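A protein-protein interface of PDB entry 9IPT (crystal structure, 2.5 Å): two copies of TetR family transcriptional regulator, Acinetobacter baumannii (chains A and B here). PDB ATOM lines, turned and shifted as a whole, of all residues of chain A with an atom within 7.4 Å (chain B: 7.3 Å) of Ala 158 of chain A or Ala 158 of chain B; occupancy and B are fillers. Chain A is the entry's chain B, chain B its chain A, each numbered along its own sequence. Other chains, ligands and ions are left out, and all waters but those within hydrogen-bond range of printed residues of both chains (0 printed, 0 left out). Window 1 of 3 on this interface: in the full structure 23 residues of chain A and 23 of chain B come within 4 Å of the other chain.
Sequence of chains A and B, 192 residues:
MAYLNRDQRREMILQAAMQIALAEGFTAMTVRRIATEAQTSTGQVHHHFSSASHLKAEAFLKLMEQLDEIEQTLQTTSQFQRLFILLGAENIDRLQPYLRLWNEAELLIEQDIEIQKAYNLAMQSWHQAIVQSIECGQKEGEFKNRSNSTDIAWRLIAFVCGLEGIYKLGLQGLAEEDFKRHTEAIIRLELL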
ATOM      1  N   LEU A  87      23.737  21.052   7.279  1.00  0.00           N
ATOM      2  CA  LEU A  87      22.935  21.374   8.452  1.00  0.00           C
ATOM      3  C   LEU A  87      22.808  20.206   9.422  1.00  0.00           C
ATOM      4  O   LEU A  87      22.183  20.362  10.476  1.00  0.00           O
ATOM      5  CB  LEU A  87      21.539  21.846   8.027  1.00  0.00           C
ATOM      6  CG  LEU A  87      21.479  23.137   7.206  1.00  0.00           C
ATOM      7  CD1 LEU A  87      20.048  23.455   6.809  1.00  0.00           C
ATOM      8  CD2 LEU A  87      22.092  24.297   7.975  1.00  0.00           C
ATOM      9  N   TRP A 126      31.152  27.180  10.138  1.00  0.00           N
ATOM     10  CA  TRP A 126      29.894  26.593   9.687  1.00  0.00           C
ATOM     11  C   TRP A 126      29.077  27.606   8.895  1.00  0.00           C
ATOM     12  O   TRP A 126      28.535  27.291   7.829  1.00  0.00           O
ATOM     13  CB  TRP A 126      29.101  26.080  10.888  1.00  0.00           C
ATOM     14  CG  TRP A 126      27.937  25.211  10.526  1.00  0.00           C
ATOM     15  CD1 TRP A 126      27.791  24.465   9.394  1.00  0.00           C
ATOM     16  CD2 TRP A 126      26.751  24.999  11.302  1.00  0.00           C
ATOM     17  NE1 TRP A 126      26.588  23.799   9.417  1.00  0.00           N
ATOM     18  CE2 TRP A 126      25.931  24.111  10.579  1.00  0.00           C
ATOM     19  CE3 TRP A 126      26.304  25.473  12.540  1.00  0.00           C
ATOM     20  CZ2 TRP A 126      24.690  23.688  11.050  1.00  0.00           C
ATOM     21  CZ3 TRP A 126      25.072  25.053  13.007  1.00  0.00           C
ATOM     22  CH2 TRP A 126      24.279  24.169  12.263  1.00  0.00           C
ATOM     23  N   ILE A 152      20.401  34.482   5.110  1.00  0.00           N
ATOM     24  CA  ILE A 152      19.799  33.160   4.980  1.00  0.00           C
ATOM     25  C   ILE A 152      20.619  32.122   5.735  1.00  0.00           C
ATOM     26  O   ILE A 152      20.066  31.209   6.360  1.00  0.00           O
ATOM     27  CB  ILE A 152      19.640  32.790   3.495  1.00  0.00           C
ATOM     28  CG1 ILE A 152      18.891  33.898   2.751  1.00  0.00           C
ATOM     29  CG2 ILE A 152      18.920  31.458   3.347  1.00  0.00           C
ATOM     30  CD1 ILE A 152      18.570  33.563   1.313  1.00  0.00           C
ATOM     31  N   ALA A 153      21.948  32.248   5.699  1.00  0.00           N
ATOM     32  CA  ALA A 153      22.800  31.296   6.405  1.00  0.00           C
ATOM     33  C   ALA A 153      22.616  31.400   7.913  1.00  0.00           C
ATOM     34  O   ALA A 153      22.550  30.380   8.608  1.00  0.00           O
ATOM     35  CB  ALA A 153      24.262  31.521   6.030  1.00  0.00           C
ATOM     36  N   TRP A 154      22.538  32.625   8.440  1.00  0.00           N
ATOM     37  CA  TRP A 154      22.293  32.795   9.868  1.00  0.00           C
ATOM     38  C   TRP A 154      20.911  32.283  10.249  1.00  0.00           C
ATOM     39  O   TRP A 154      20.732  31.687  11.318  1.00  0.00           O
ATOM     40  CB  TRP A 154      22.447  34.265  10.258  1.00  0.00           C
ATOM     41  CG  TRP A 154      23.870  34.702  10.465  1.00  0.00           C
ATOM     42  CD1 TRP A 154      24.490  35.768   9.878  1.00  0.00           C
ATOM     43  CD2 TRP A 154      24.845  34.098  11.327  1.00  0.00           C
ATOM     44  NE1 TRP A 154      25.790  35.860  10.313  1.00  0.00           N
ATOM     45  CE2 TRP A 154      26.033  34.848  11.203  1.00  0.00           C
ATOM     46  CE3 TRP A 154      24.831  32.995  12.188  1.00  0.00           C
ATOM     47  CZ2 TRP A 154      27.193  34.530  11.908  1.00  0.00           C
ATOM     48  CZ3 TRP A 154      25.985  32.682  12.885  1.00  0.00           C
ATOM     49  CH2 TRP A 154      27.149  33.447  12.741  1.00  0.00           C
ATOM     50  N   ARG A 155      19.917  32.503   9.384  1.00  0.00           N
ATOM     51  CA  ARG A 155      18.568  32.030   9.671  1.00  0.00           C
ATOM     52  C   ARG A 155      18.491  30.509   9.613  1.00  0.00           C
ATOM     53  O   ARG A 155      17.761  29.889  10.394  1.00  0.00           O
ATOM     54  CB  ARG A 155      17.574  32.654   8.694  1.00  0.00           C
ATOM     55  CG  ARG A 155      16.981  33.969   9.168  1.00  0.00           C
ATOM     56  CD  ARG A 155      15.979  34.514   8.163  1.00  0.00           C
ATOM     57  NE  ARG A 155      16.332  35.856   7.718  1.00  0.00           N
ATOM     58  CZ  ARG A 155      16.356  36.244   6.451  1.00  0.00           C
ATOM     59  NH1 ARG A 155      16.046  35.413   5.469  1.00  0.00           N
ATOM     60  NH2 ARG A 155      16.697  37.496   6.162  1.00  0.00           N
ATOM     61  N   LEU A 156      19.233  29.893   8.691  1.00  0.00           N
ATOM     62  CA  LEU A 156      19.246  28.436   8.612  1.00  0.00           C
ATOM     63  C   LEU A 156      19.938  27.825   9.824  1.00  0.00           C
ATOM     64  O   LEU A 156      19.467  26.824  10.374  1.00  0.00           O
ATOM     65  CB  LEU A 156      19.926  27.982   7.321  1.00  0.00           C
ATOM     66  CG  LEU A 156      19.131  28.167   6.028  1.00  0.00           C
ATOM     67  CD1 LEU A 156      19.844  27.493   4.865  1.00  0.00           C
ATOM     68  CD2 LEU A 156      17.719  27.626   6.184  1.00  0.00           C
ATOM     69  N   ILE A 157      21.057  28.415  10.252  1.00  0.00           N
ATOM     70  CA  ILE A 157      21.753  27.921  11.437  1.00  0.00           C
ATOM     71  C   ILE A 157      20.886  28.108  12.676  1.00  0.00           C
ATOM     72  O   ILE A 157      20.828  27.237  13.552  1.00  0.00           O
ATOM     73  CB  ILE A 157      23.119  28.621  11.582  1.00  0.00           C
ATOM     74  CG1 ILE A 157      24.206  27.822  10.865  1.00  0.00           C
ATOM     75  CG2 ILE A 157      23.491  28.804  13.045  1.00  0.00           C
ATOM     76  CD1 ILE A 157      25.461  28.616  10.603  1.00  0.00           C
ATOM     77  N   ALA A 158      20.186  29.241  12.762  1.00  0.00           N
ATOM     78  CA  ALA A 158      19.348  29.501  13.927  1.00  0.00           C
ATOM     79  C   ALA A 158      18.146  28.566  13.980  1.00  0.00           C
ATOM     80  O   ALA A 158      17.648  28.264  15.070  1.00  0.00           O
ATOM     81  CB  ALA A 158      18.887  30.959  13.931  1.00  0.00           C
ATOM     82  N   PHE A 159      17.670  28.095  12.827  1.00  0.00           N
ATOM     83  CA  PHE A 159      16.506  27.216  12.823  1.00  0.00           C
ATOM     84  C   PHE A 159      16.869  25.804  13.266  1.00  0.00           C
ATOM     85  O   PHE A 159      16.162  25.202  14.080  1.00  0.00           O
ATOM     86  CB  PHE A 159      15.859  27.188  11.438  1.00  0.00           C
ATOM     87  CG  PHE A 159      14.690  26.247  11.342  1.00  0.00           C
ATOM     88  CD1 PHE A 159      13.442  26.626  11.809  1.00  0.00           C
ATOM     89  CD2 PHE A 159      14.842  24.980  10.801  1.00  0.00           C
ATOM     90  CE1 PHE A 159      12.366  25.761  11.732  1.00  0.00           C
ATOM     91  CE2 PHE A 159      13.769  24.112  10.722  1.00  0.00           C
ATOM     92  CZ  PHE A 159      12.530  24.502  11.188  1.00  0.00           C
ATOM     93  N   VAL A 160      17.963  25.254  12.732  1.00  0.00           N
ATOM     94  CA  VAL A 160      18.344  23.889  13.081  1.00  0.00           C
ATOM     95  C   VAL A 160      18.776  23.813  14.539  1.00  0.00           C
ATOM     96  O   VAL A 160      18.483  22.834  15.236  1.00  0.00           O
ATOM     97  CB  VAL A 160      19.441  23.369  12.133  1.00  0.00           C
ATOM     98  CG1 VAL A 160      18.862  23.092  10.753  1.00  0.00           C
ATOM     99  CG2 VAL A 160      20.600  24.351  12.049  1.00  0.00           C
ATOM    100  N   CYS A 161      19.472  24.843  15.027  1.00  0.00           N
ATOM    101  CA  CYS A 161      19.850  24.875  16.435  1.00  0.00           C
ATOM    102  C   CYS A 161      18.623  24.989  17.328  1.00  0.00           C
ATOM    103  O   CYS A 161      18.564  24.371  18.397  1.00  0.00           O
ATOM    104  CB  CYS A 161      20.814  26.033  16.695  1.00  0.00           C
ATOM    105  SG  CYS A 161      22.545  25.664  16.331  1.00  0.00           S
ATOM    106  N   GLY A 162      17.628  25.770  16.902  1.00  0.00           N
ATOM    107  CA  GLY A 162      16.415  25.901  17.688  1.00  0.00           C
ATOM    108  C   GLY A 162      15.519  24.684  17.612  1.00  0.00           C
ATOM    109  O   GLY A 162      14.853  24.342  18.591  1.00  0.00           O
ATOM    110  N   LEU A 163      15.490  24.013  16.459  1.00  0.00           N
ATOM    111  CA  LEU A 163      14.655  22.825  16.324  1.00  0.00           C
ATOM    112  C   LEU A 163      15.178  21.682  17.182  1.00  0.00           C
ATOM    113  O   LEU A 163      14.396  20.984  17.840  1.00  0.00           O
ATOM    114  CB  LEU A 163      14.572  22.403  14.858  1.00  0.00           C
ATOM    115  CG  LEU A 163      13.491  21.377  14.515  1.00  0.00           C
ATOM    116  CD1 LEU A 163      12.227  21.613  15.334  1.00  0.00           C
ATOM    117  CD2 LEU A 163      13.184  21.409  13.030  1.00  0.00           C
ATOM    118  N   GLU A 164      16.497  21.470  17.188  1.00  0.00           N
ATOM    119  CA  GLU A 164      17.072  20.431  18.035  1.00  0.00           C
ATOM    120  C   GLU A 164      16.888  20.748  19.513  1.00  0.00           C
ATOM    121  O   GLU A 164      16.788  19.830  20.335  1.00  0.00           O
ATOM    122  CB  GLU A 164      18.556  20.246  17.713  1.00  0.00           C
ATOM    123  CG  GLU A 164      19.066  18.828  17.926  1.00  0.00           C
ATOM    124  CD  GLU A 164      19.012  17.991  16.661  1.00  0.00           C
ATOM    125  OE1 GLU A 164      19.580  18.423  15.635  1.00  0.00           O
ATOM    126  OE2 GLU A 164      18.402  16.901  16.690  1.00  0.00           O
ATOM    127  N   GLY A 165      16.837  22.033  19.869  1.00  0.00           N
ATOM    128  CA  GLY A 165      16.627  22.397  21.260  1.00  0.00           C
ATOM    129  C   GLY A 165      15.221  22.091  21.742  1.00  0.00           C
ATOM    130  O   GLY A 165      15.030  21.627  22.869  1.00  0.00           O
ATOM    131  N   ILE A 166      14.218  22.350  20.898  1.00  0.00           N
ATOM    132  CA  ILE A 166      12.838  22.044  21.265  1.00  0.00           C
ATOM    133  C   ILE A 166      12.648  20.544  21.438  1.00  0.00           C
ATOM    134  O   ILE A 166      11.848  20.101  22.273  1.00  0.00           O
ATOM    135  CB  ILE A 166      11.867  22.621  20.215  1.00  0.00           C
ATOM    136  CG1 ILE A 166      12.089  24.125  20.055  1.00  0.00           C
ATOM    137  CG2 ILE A 166      10.422  22.345  20.601  1.00  0.00           C
ATOM    138  CD1 ILE A 166      11.782  24.919  21.301  1.00  0.00           C
ATOM    139  N   HIS A 182      10.970  19.481   8.456  1.00  0.00           N
ATOM    140  CA  HIS A 182      10.949  20.912   8.750  1.00  0.00           C
ATOM    141  C   HIS A 182      12.153  21.620   8.146  1.00  0.00           C
ATOM    142  O   HIS A 182      12.035  22.754   7.664  1.00  0.00           O
ATOM    143  CB  HIS A 182      10.895  21.141  10.259  1.00  0.00           C
ATOM    144  CG  HIS A 182       9.591  20.753  10.882  1.00  0.00           C
ATOM    145  ND1 HIS A 182       8.400  21.365  10.556  1.00  0.00           N
ATOM    146  CD2 HIS A 182       9.293  19.825  11.822  1.00  0.00           C
ATOM    147  CE1 HIS A 182       7.422  20.825  11.261  1.00  0.00           C
ATOM    148  NE2 HIS A 182       7.937  19.887  12.036  1.00  0.00           N
ATOM    149  N   LEU B  87       5.052  35.686  19.720  1.00  0.00           N
ATOM    150  CA  LEU B  87       6.351  35.026  19.707  1.00  0.00           C
ATOM    151  C   LEU B  87       7.332  35.624  20.705  1.00  0.00           C
ATOM    152  O   LEU B  87       8.454  35.120  20.822  1.00  0.00           O
ATOM    153  CB  LEU B  87       6.957  35.086  18.302  1.00  0.00           C
ATOM    154  CG  LEU B  87       6.314  34.212  17.225  1.00  0.00           C
ATOM    155  CD1 LEU B  87       6.603  34.783  15.848  1.00  0.00           C
ATOM    156  CD2 LEU B  87       6.818  32.784  17.326  1.00  0.00           C
ATOM    157  N   TRP B 126       1.794  27.881  24.666  1.00  0.00           N
ATOM    158  CA  TRP B 126       2.369  28.851  23.740  1.00  0.00           C
ATOM    159  C   TRP B 126       2.220  28.387  22.297  1.00  0.00           C
ATOM    160  O   TRP B 126       2.010  29.203  21.391  1.00  0.00           O
ATOM    161  CB  TRP B 126       3.842  29.082  24.078  1.00  0.00           C
ATOM    162  CG  TRP B 126       4.490  30.178  23.287  1.00  0.00           C
ATOM    163  CD1 TRP B 126       3.896  31.310  22.812  1.00  0.00           C
ATOM    164  CD2 TRP B 126       5.863  30.244  22.881  1.00  0.00           C
ATOM    165  NE1 TRP B 126       4.813  32.077  22.135  1.00  0.00           N
ATOM    166  CE2 TRP B 126       6.028  31.444  22.162  1.00  0.00           C
ATOM    167  CE3 TRP B 126       6.967  29.405  23.055  1.00  0.00           C
ATOM    168  CZ2 TRP B 126       7.253  31.826  21.618  1.00  0.00           C
ATOM    169  CZ3 TRP B 126       8.182  29.784  22.513  1.00  0.00           C
ATOM    170  CH2 TRP B 126       8.315  30.983  21.804  1.00  0.00           C
ATOM    171  N   ILE B 152       3.633  25.248  11.015  1.00  0.00           N
ATOM    172  CA  ILE B 152       4.119  26.627  11.027  1.00  0.00           C
ATOM    173  C   ILE B 152       4.446  27.057  12.448  1.00  0.00           C
ATOM    174  O   ILE B 152       5.478  27.689  12.701  1.00  0.00           O
ATOM    175  CB  ILE B 152       3.092  27.580  10.384  1.00  0.00           C
ATOM    176  CG1 ILE B 152       2.480  26.974   9.121  1.00  0.00           C
ATOM    177  CG2 ILE B 152       3.738  28.925  10.076  1.00  0.00           C
ATOM    178  CD1 ILE B 152       3.288  27.200   7.874  1.00  0.00           C
ATOM    179  N   ALA B 153       3.574  26.716  13.398  1.00  0.00           N
ATOM    180  CA  ALA B 153       3.762  27.160  14.775  1.00  0.00           C
ATOM    181  C   ALA B 153       5.023  26.564  15.386  1.00  0.00           C
ATOM    182  O   ALA B 153       5.749  27.252  16.114  1.00  0.00           O
ATOM    183  CB  ALA B 153       2.534  26.799  15.609  1.00  0.00           C
ATOM    184  N   TRP B 154       5.310  25.291  15.100  1.00  0.00           N
ATOM    185  CA  TRP B 154       6.499  24.665  15.669  1.00  0.00           C
ATOM    186  C   TRP B 154       7.771  25.229  15.050  1.00  0.00           C
ATOM    187  O   TRP B 154       8.777  25.411  15.746  1.00  0.00           O
ATOM    188  CB  TRP B 154       6.437  23.147  15.490  1.00  0.00           C
ATOM    189  CG  TRP B 154       5.556  22.445  16.492  1.00  0.00           C
ATOM    190  CD1 TRP B 154       4.629  21.480  16.225  1.00  0.00           C
ATOM    191  CD2 TRP B 154       5.527  22.642  17.916  1.00  0.00           C
ATOM    192  NE1 TRP B 154       4.020  21.071  17.385  1.00  0.00           N
ATOM    193  CE2 TRP B 154       4.554  21.766  18.438  1.00  0.00           C
ATOM    194  CE3 TRP B 154       6.227  23.472  18.799  1.00  0.00           C
ATOM    195  CZ2 TRP B 154       4.255  21.704  19.798  1.00  0.00           C
ATOM    196  CZ3 TRP B 154       5.934  23.404  20.149  1.00  0.00           C
ATOM    197  CH2 TRP B 154       4.958  22.525  20.635  1.00  0.00           C
ATOM    198  N   ARG B 155       7.748  25.513  13.747  1.00  0.00           N
ATOM    199  CA  ARG B 155       8.913  26.114  13.106  1.00  0.00           C
ATOM    200  C   ARG B 155       9.105  27.557  13.556  1.00  0.00           C
ATOM    201  O   ARG B 155      10.242  28.026  13.687  1.00  0.00           O
ATOM    202  CB  ARG B 155       8.777  26.036  11.586  1.00  0.00           C
ATOM    203  CG  ARG B 155       8.804  24.619  11.039  1.00  0.00           C
ATOM    204  CD  ARG B 155       9.053  24.605   9.541  1.00  0.00           C
ATOM    205  NE  ARG B 155       8.003  25.299   8.807  1.00  0.00           N
ATOM    206  CZ  ARG B 155       6.993  24.696   8.194  1.00  0.00           C
ATOM    207  NH1 ARG B 155       6.858  23.381   8.214  1.00  0.00           N
ATOM    208  NH2 ARG B 155       6.098  25.432   7.541  1.00  0.00           N
ATOM    209  N   LEU B 156       8.006  28.276  13.796  1.00  0.00           N
ATOM    210  CA  LEU B 156       8.115  29.642  14.300  1.00  0.00           C
ATOM    211  C   LEU B 156       8.680  29.660  15.715  1.00  0.00           C
ATOM    212  O   LEU B 156       9.502  30.521  16.050  1.00  0.00           O
ATOM    213  CB  LEU B 156       6.751  30.330  14.257  1.00  0.00           C
ATOM    214  CG  LEU B 156       6.239  30.797  12.892  1.00  0.00           C
ATOM    215  CD1 LEU B 156       5.235  31.925  13.062  1.00  0.00           C
ATOM    216  CD2 LEU B 156       7.386  31.225  11.986  1.00  0.00           C
ATOM    217  N   ILE B 157       8.250  28.721  16.560  1.00  0.00           N
ATOM    218  CA  ILE B 157       8.794  28.631  17.911  1.00  0.00           C
ATOM    219  C   ILE B 157      10.262  28.223  17.866  1.00  0.00           C
ATOM    220  O   ILE B 157      11.096  28.767  18.599  1.00  0.00           O
ATOM    221  CB  ILE B 157       7.956  27.655  18.758  1.00  0.00           C
ATOM    222  CG1 ILE B 157       6.727  28.365  19.326  1.00  0.00           C
ATOM    223  CG2 ILE B 157       8.790  27.055  19.882  1.00  0.00           C
ATOM    224  CD1 ILE B 157       5.586  27.433  19.648  1.00  0.00           C
ATOM    225  N   ALA B 158      10.601  27.268  16.997  1.00  0.00           N
ATOM    226  CA  ALA B 158      11.984  26.816  16.893  1.00  0.00           C
ATOM    227  C   ALA B 158      12.902  27.923  16.397  1.00  0.00           C
ATOM    228  O   ALA B 158      14.083  27.959  16.764  1.00  0.00           O
ATOM    229  CB  ALA B 158      12.071  25.601  15.970  1.00  0.00           C
ATOM    230  N   PHE B 159      12.387  28.836  15.573  1.00  0.00           N
ATOM    231  CA  PHE B 159      13.226  29.904  15.042  1.00  0.00           C
ATOM    232  C   PHE B 159      13.491  30.979  16.090  1.00  0.00           C
ATOM    233  O   PHE B 159      14.633  31.420  16.256  1.00  0.00           O
ATOM    234  CB  PHE B 159      12.582  30.519  13.798  1.00  0.00           C
ATOM    235  CG  PHE B 159      13.393  31.626  13.189  1.00  0.00           C
ATOM    236  CD1 PHE B 159      14.496  31.340  12.403  1.00  0.00           C
ATOM    237  CD2 PHE B 159      13.065  32.951  13.417  1.00  0.00           C
ATOM    238  CE1 PHE B 159      15.251  32.354  11.848  1.00  0.00           C
ATOM    239  CE2 PHE B 159      13.815  33.971  12.865  1.00  0.00           C
ATOM    240  CZ  PHE B 159      14.909  33.671  12.079  1.00  0.00           C
ATOM    241  N   VAL B 160      12.449  31.418  16.801  1.00  0.00           N
ATOM    242  CA  VAL B 160      12.638  32.465  17.800  1.00  0.00           C
ATOM    243  C   VAL B 160      13.439  31.943  18.987  1.00  0.00           C
ATOM    244  O   VAL B 160      14.225  32.687  19.586  1.00  0.00           O
ATOM    245  CB  VAL B 160      11.281  33.057  18.236  1.00  0.00           C
ATOM    246  CG1 VAL B 160      10.493  33.528  17.021  1.00  0.00           C
ATOM    247  CG2 VAL B 160      10.469  32.044  19.031  1.00  0.00           C
ATOM    248  N   CYS B 161      13.269  30.667  19.342  1.00  0.00           N
ATOM    249  CA  CYS B 161      14.100  30.083  20.387  1.00  0.00           C
ATOM    250  C   CYS B 161      15.520  29.852  19.892  1.00  0.00           C
ATOM    251  O   CYS B 161      16.475  29.970  20.668  1.00  0.00           O
ATOM    252  CB  CYS B 161      13.490  28.770  20.880  1.00  0.00           C
ATOM    253  SG  CYS B 161      12.325  28.947  22.251  1.00  0.00           S
ATOM    254  N   GLY B 162      15.676  29.532  18.608  1.00  0.00           N
ATOM    255  CA  GLY B 162      17.006  29.315  18.065  1.00  0.00           C
ATOM    256  C   GLY B 162      17.772  30.606  17.865  1.00  0.00           C
ATOM    257  O   GLY B 162      18.981  30.660  18.103  1.00  0.00           O
ATOM    258  N   LEU B 163      17.085  31.662  17.424  1.00  0.00           N
ATOM    259  CA  LEU B 163      17.761  32.939  17.225  1.00  0.00           C
ATOM    260  C   LEU B 163      18.251  33.525  18.542  1.00  0.00           C
ATOM    261  O   LEU B 163      19.297  34.181  18.574  1.00  0.00           O
ATOM    262  CB  LEU B 163      16.831  33.922  16.516  1.00  0.00           C
ATOM    263  CG  LEU B 163      17.528  35.091  15.816  1.00  0.00           C
ATOM    264  CD1 LEU B 163      18.568  34.578  14.833  1.00  0.00           C
ATOM    265  CD2 LEU B 163      16.516  35.980  15.112  1.00  0.00           C
ATOM    266  N   GLU B 164      17.529  33.241  19.621  1.00  0.00           N
ATOM    267  CA  GLU B 164      17.906  33.719  20.943  1.00  0.00           C
ATOM    268  C   GLU B 164      19.170  33.011  21.427  1.00  0.00           C
ATOM    269  O   GLU B 164      20.027  33.625  22.062  1.00  0.00           O
ATOM    270  CB  GLU B 164      16.765  33.502  21.938  1.00  0.00           C
ATOM    271  CG  GLU B 164      16.074  34.782  22.379  1.00  0.00           C
ATOM    272  CD  GLU B 164      14.564  34.651  22.402  1.00  0.00           C
ATOM    273  OE1 GLU B 164      14.066  33.528  22.633  1.00  0.00           O
ATOM    274  OE2 GLU B 164      13.874  35.670  22.191  1.00  0.00           O
ATOM    275  N   GLY B 165      19.282  31.720  21.125  1.00  0.00           N
ATOM    276  CA  GLY B 165      20.444  30.947  21.529  1.00  0.00           C
ATOM    277  C   GLY B 165      21.708  31.359  20.797  1.00  0.00           C
ATOM    278  O   GLY B 165      22.794  31.381  21.384  1.00  0.00           O
ATOM    279  N   ILE B 166      21.587  31.689  19.509  1.00  0.00           N
ATOM    280  CA  ILE B 166      22.747  32.152  18.756  1.00  0.00           C
ATOM    281  C   ILE B 166      23.195  33.529  19.228  1.00  0.00           C
ATOM    282  O   ILE B 166      24.364  33.896  19.053  1.00  0.00           O
ATOM    283  CB  ILE B 166      22.444  32.153  17.244  1.00  0.00           C
ATOM    284  CG1 ILE B 166      21.763  30.843  16.843  1.00  0.00           C
ATOM    285  CG2 ILE B 166      23.719  32.354  16.437  1.00  0.00           C
ATOM    286  CD1 ILE B 166      22.719  29.736  16.466  1.00  0.00           C
ATOM    287  N   LEU B 174      27.288  38.755  13.510  1.00  0.00           N
ATOM    288  CA  LEU B 174      25.854  38.781  13.731  1.00  0.00           C
ATOM    289  C   LEU B 174      25.498  40.045  14.506  1.00  0.00           C
ATOM    290  O   LEU B 174      26.255  40.495  15.372  1.00  0.00           O
ATOM    291  CB  LEU B 174      25.406  37.542  14.507  1.00  0.00           C
ATOM    292  CG  LEU B 174      24.072  36.898  14.110  1.00  0.00           C
ATOM    293  CD1 LEU B 174      23.922  35.509  14.765  1.00  0.00           C
ATOM    294  CD2 LEU B 174      22.835  37.797  14.310  1.00  0.00           C
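The guanidinium group of Arg 155 of chain B lies close to a ring nitrogen (ND1) of His 182 of chain A (3.5 Å).
O of Ile 157 of chain A sits close to SG of Cys 161 of chain A, 3.6 Å away.
Among the printed residues, pairs that only touch across the chains: Ala 158 of chain A with Gly 162 of chain B (3.2 Å), Gly 162 of chain A with Ala 158 of chain B (3.2 Å), Gly 162 of chain A with Gly 162 of chain B (3.5 Å), Arg 155 of chain A with Phe 159 of chain B (3.6 Å), Phe 159 of chain A with Arg 155 of chain B (3.6 Å), Ile 157 of chain A with Ile 166 of chain B (3.6 Å), Trp 154 of chain A with Leu 174 of chain B (3.7 Å), Ala 158 of chain A with Leu 163 of chain B (3.7 Å), Leu 163 of chain A with Ala 158 of chain B (3.8 Å), Ile 166 of chain A with Ile 157 of chain B (3.9 Å) and Ala 158 of chain A with Ala 158 of chain B (3.96 Å).
Leu 87 of chain A touches none of the printed residues of chain B. Printed residues of chain B within 4 Å of Ala 158 of chain A: Ala 158, Gly 162 and Leu 163. Printed residues of chain B within 4 Å of Ile 166 of chain A: Ile 157 (3.9 Å). Of the printed residues of chain A, Arg 155 of chain B touches Phe 159 and His 182. Of the printed residues of chain A, Ile 157 of chain B touches Ile 166 (3.9 Å). Ala 158 of chain B touches just these residues of chain A: Ala 158, Gly 162 and Leu 163. Of the printed residues of chain A, Leu 163 of chain B touches Ala 158 (3.7 Å). Printed residues of chain A within 4 Å of Ile 166 of chain B: Ile 157 (3.6 Å).
Hydrophobic or aromatic side chains of chain A within 4 Å of the printed part of chain B: Trp 154, Ile 157, Ala 158, Phe 159, Ile 166 and His 182. Along chain A the printed residues that touch a printed residue of chain B span positions 154 to 182. Of the 18 printed residues of chain B, 8 touch a printed residue of chain A. Among the printed residues, no Asp or Glu carboxylate lies within 4 Å of a Lys or Arg side-chain nitrogen of the other chain.
Arg 155 of chain A touches Phe 159 of chain B, and with the chains exchanged Phe 159 of chain A touches Arg 155 of chain B. Ala 158 of chain A touches Gly 162 of chain B, and with the chains exchanged Gly 162 of chain A touches Ala 158 of chain B. Ala 158 of chain A touches Leu 163 of chain B, and with the chains exchanged Leu 163 of chain A touches Ala 158 of chain B. Gly 162 of chain A touches its own counterpart, Gly 162 of chain B. Of the 12 pairs that touch across the chains among the printed residues, 10 have their exchanged pair printed and touching as well.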
